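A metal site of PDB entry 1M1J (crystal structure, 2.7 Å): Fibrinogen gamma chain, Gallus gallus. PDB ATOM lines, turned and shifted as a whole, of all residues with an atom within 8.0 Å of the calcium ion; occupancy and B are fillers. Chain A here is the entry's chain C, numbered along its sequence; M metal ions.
The side-chain carboxylate (OD2) of Asp 320 is in hydrogen-bond range of the backbone NH (N) of Cys 326 (3.0 Å).
The backbone NH (N) of Asp 320 sits at hydrogen-bond distance from the side-chain hydroxyl (OG) of Ser 313.
The nearest printed residue that does not touch the calcium ion is Glu 323 (4.1 Å).
The calcium ion is bound by the backbone carbonyl oxygen (O) of Phe 322 (2.2 Å), the backbone carbonyl oxygen (O) of Gly 324 (2.3 Å), the side-chain carboxylate (OD1) of Asp 320 (2.4 Å), the side-chain carboxylate (OD2) of Asp 318 (2.4 Å) and the side-chain carboxylate (OD1) of Asp 318 (2.6 Å).
The calcium ion has five donor atoms within binding distance.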
ATOM      1  N   SER A 313     -33.702  -3.439  13.648  1.00  0.00           N
ATOM      2  CA  SER A 313     -32.377  -3.996  13.878  1.00  0.00           C
ATOM      3  C   SER A 313     -31.904  -3.884  15.308  1.00  0.00           C
ATOM      4  O   SER A 313     -32.145  -2.870  15.968  1.00  0.00           O
ATOM      5  CB  SER A 313     -31.328  -3.321  12.962  1.00  0.00           C
ATOM      6  OG  SER A 313     -31.446  -3.746  11.610  1.00  0.00           O
ATOM      7  N   ASN A 317     -29.158  -8.877  15.484  1.00  0.00           N
ATOM      8  CA  ASN A 317     -30.047  -9.154  14.347  1.00  0.00           C
ATOM      9  C   ASN A 317     -29.962  -7.935  13.426  1.00  0.00           C
ATOM     10  O   ASN A 317     -30.779  -7.017  13.516  1.00  0.00           O
ATOM     11  CB  ASN A 317     -31.477  -9.378  14.838  1.00  0.00           C
ATOM     12  CG  ASN A 317     -32.344 -10.166  13.859  1.00  0.00           C
ATOM     13  OD1 ASN A 317     -33.078 -11.065  14.271  1.00  0.00           O
ATOM     14  ND2 ASN A 317     -32.264  -9.836  12.573  1.00  0.00           N
ATOM     15  N   ASP A 318     -28.937  -7.930  12.566  1.00  0.00           N
ATOM     16  CA  ASP A 318     -28.668  -6.834  11.638  1.00  0.00           C
ATOM     17  C   ASP A 318     -29.538  -6.884  10.387  1.00  0.00           C
ATOM     18  O   ASP A 318     -29.489  -7.850   9.619  1.00  0.00           O
ATOM     19  CB  ASP A 318     -27.186  -6.876  11.210  1.00  0.00           C
ATOM     20  CG  ASP A 318     -26.747  -5.650  10.433  1.00  0.00           C
ATOM     21  OD1 ASP A 318     -27.517  -5.168   9.572  1.00  0.00           O
ATOM     22  OD2 ASP A 318     -25.627  -5.160  10.674  1.00  0.00           O
ATOM     23  N   ASN A 319     -30.338  -5.845  10.167  1.00  0.00           N
ATOM     24  CA  ASN A 319     -31.147  -5.807   8.971  1.00  0.00           C
ATOM     25  C   ASN A 319     -31.076  -4.432   8.332  1.00  0.00           C
ATOM     26  O   ASN A 319     -31.994  -4.030   7.608  1.00  0.00           O
ATOM     27  CB  ASN A 319     -32.596  -6.183   9.288  1.00  0.00           C
ATOM     28  CG  ASN A 319     -32.697  -7.525   9.984  1.00  0.00           C
ATOM     29  OD1 ASN A 319     -32.498  -7.625  11.194  1.00  0.00           O
ATOM     30  ND2 ASN A 319     -32.994  -8.572   9.230  1.00  0.00           N
ATOM     31  N   ASP A 320     -30.004  -3.705   8.601  1.00  0.00           N
ATOM     32  CA  ASP A 320     -29.842  -2.367   8.043  1.00  0.00           C
ATOM     33  C   ASP A 320     -29.245  -2.394   6.634  1.00  0.00           C
ATOM     34  O   ASP A 320     -29.086  -3.451   6.028  1.00  0.00           O
ATOM     35  CB  ASP A 320     -28.982  -1.504   8.959  1.00  0.00           C
ATOM     36  CG  ASP A 320     -27.624  -2.107   9.225  1.00  0.00           C
ATOM     37  OD1 ASP A 320     -26.989  -2.605   8.262  1.00  0.00           O
ATOM     38  OD2 ASP A 320     -27.167  -2.061  10.385  1.00  0.00           O
ATOM     39  N   ASN A 321     -28.926  -1.216   6.106  1.00  0.00           N
ATOM     40  CA  ASN A 321     -28.315  -1.113   4.784  1.00  0.00           C
ATOM     41  C   ASN A 321     -26.884  -0.678   4.952  1.00  0.00           C
ATOM     42  O   ASN A 321     -26.331   0.007   4.104  1.00  0.00           O
ATOM     43  CB  ASN A 321     -29.027  -0.085   3.902  1.00  0.00           C
ATOM     44  CG  ASN A 321     -30.411  -0.526   3.515  1.00  0.00           C
ATOM     45  OD1 ASN A 321     -30.631  -1.674   3.115  1.00  0.00           O
ATOM     46  ND2 ASN A 321     -31.366   0.402   3.623  1.00  0.00           N
ATOM     47  N   PHE A 322     -26.287  -1.061   6.069  1.00  0.00           N
ATOM     48  CA  PHE A 322     -24.895  -0.722   6.333  1.00  0.00           C
ATOM     49  C   PHE A 322     -24.028  -1.996   6.380  1.00  0.00           C
ATOM     50  O   PHE A 322     -24.440  -3.008   6.909  1.00  0.00           O
ATOM     51  CB  PHE A 322     -24.842   0.025   7.666  1.00  0.00           C
ATOM     52  CG  PHE A 322     -23.469   0.415   8.093  1.00  0.00           C
ATOM     53  CD1 PHE A 322     -22.569   1.007   7.197  1.00  0.00           C
ATOM     54  CD2 PHE A 322     -23.081   0.244   9.419  1.00  0.00           C
ATOM     55  CE1 PHE A 322     -21.308   1.421   7.613  1.00  0.00           C
ATOM     56  CE2 PHE A 322     -21.813   0.656   9.854  1.00  0.00           C
ATOM     57  CZ  PHE A 322     -20.920   1.250   8.938  1.00  0.00           C
ATOM     58  N   GLU A 323     -22.828  -1.923   5.799  1.00  0.00           N
ATOM     59  CA  GLU A 323     -21.908  -3.068   5.781  1.00  0.00           C
ATOM     60  C   GLU A 323     -21.605  -3.423   7.239  1.00  0.00           C
ATOM     61  O   GLU A 323     -21.337  -4.585   7.575  1.00  0.00           O
ATOM     62  CB  GLU A 323     -20.605  -2.717   5.020  1.00  0.00           C
ATOM     63  CG  GLU A 323     -19.955  -1.395   5.443  1.00  0.00           C
ATOM     64  CD  GLU A 323     -20.360  -0.214   4.570  1.00  0.00           C
ATOM     65  OE1 GLU A 323     -21.468  -0.243   4.003  1.00  0.00           O
ATOM     66  OE2 GLU A 323     -19.571   0.753   4.479  1.00  0.00           O
ATOM     67  N   GLY A 324     -21.649  -2.398   8.088  1.00  0.00           N
ATOM     68  CA  GLY A 324     -21.431  -2.600   9.501  1.00  0.00           C
ATOM     69  C   GLY A 324     -22.752  -2.856  10.196  1.00  0.00           C
ATOM     70  O   GLY A 324     -23.761  -3.183   9.554  1.00  0.00           O
ATOM     71  N   ASN A 325     -22.760  -2.707  11.522  1.00  0.00           N
ATOM     72  CA  ASN A 325     -23.961  -2.928  12.318  1.00  0.00           C
ATOM     73  C   ASN A 325     -24.419  -1.662  13.067  1.00  0.00           C
ATOM     74  O   ASN A 325     -23.992  -1.427  14.199  1.00  0.00           O
ATOM     75  CB  ASN A 325     -23.683  -4.039  13.330  1.00  0.00           C
ATOM     76  CG  ASN A 325     -24.917  -4.441  14.123  1.00  0.00           C
ATOM     77  OD1 ASN A 325     -24.916  -5.470  14.784  1.00  0.00           O
ATOM     78  ND2 ASN A 325     -25.980  -3.631  14.071  1.00  0.00           N
ATOM     79  N   CYS A 326     -25.305  -0.868  12.459  1.00  0.00           N
ATOM     80  CA  CYS A 326     -25.809   0.369  13.103  1.00  0.00           C
ATOM     81  C   CYS A 326     -26.268   0.135  14.546  1.00  0.00           C
ATOM     82  O   CYS A 326     -25.785   0.776  15.490  1.00  0.00           O
ATOM     83  CB  CYS A 326     -26.960   0.999  12.299  1.00  0.00           C
ATOM     84  SG  CYS A 326     -26.546   1.597  10.623  1.00  0.00           S
ATOM     85  N   ALA A 327     -27.189  -0.803  14.719  1.00  0.00           N
ATOM     86  CA  ALA A 327     -27.712  -1.118  16.055  1.00  0.00           C
ATOM     87  C   ALA A 327     -26.607  -1.409  17.061  1.00  0.00           C
ATOM     88  O   ALA A 327     -26.658  -0.955  18.208  1.00  0.00           O
ATOM     89  CB  ALA A 327     -28.678  -2.304  15.965  1.00  0.00           C
ATOM     90  N   MET A 336     -32.894   0.902  11.542  1.00  0.00           N
ATOM     91  CA  MET A 336     -31.693   1.474  10.933  1.00  0.00           C
ATOM     92  C   MET A 336     -31.629   1.330   9.416  1.00  0.00           C
ATOM     93  O   MET A 336     -32.071   0.313   8.867  1.00  0.00           O
ATOM     94  CB  MET A 336     -30.471   0.812  11.558  1.00  0.00           C
ATOM     95  CG  MET A 336     -30.442   0.906  13.067  1.00  0.00           C
ATOM     96  SD  MET A 336     -30.287   2.604  13.596  1.00  0.00           S
ATOM     97  CE  MET A 336     -29.391   2.416  15.137  1.00  0.00           C
ATOM     98  N   ASN A 337     -31.089   2.363   8.760  1.00  0.00           N
ATOM     99  CA  ASN A 337     -30.902   2.399   7.289  1.00  0.00           C
ATOM    100  C   ASN A 337     -29.360   2.337   7.147  1.00  0.00           C
ATOM    101  O   ASN A 337     -28.762   1.303   7.438  1.00  0.00           O
ATOM    102  CB  ASN A 337     -31.434   3.729   6.738  1.00  0.00           C
ATOM    103  CG  ASN A 337     -31.497   3.765   5.216  1.00  0.00           C
ATOM    104  OD1 ASN A 337     -30.648   3.201   4.532  1.00  0.00           O
ATOM    105  ND2 ASN A 337     -32.505   4.461   4.681  1.00  0.00           N
HETATM  106 CA    CA M   1     -25.369  -4.383   8.393  1.00  0.00          CA
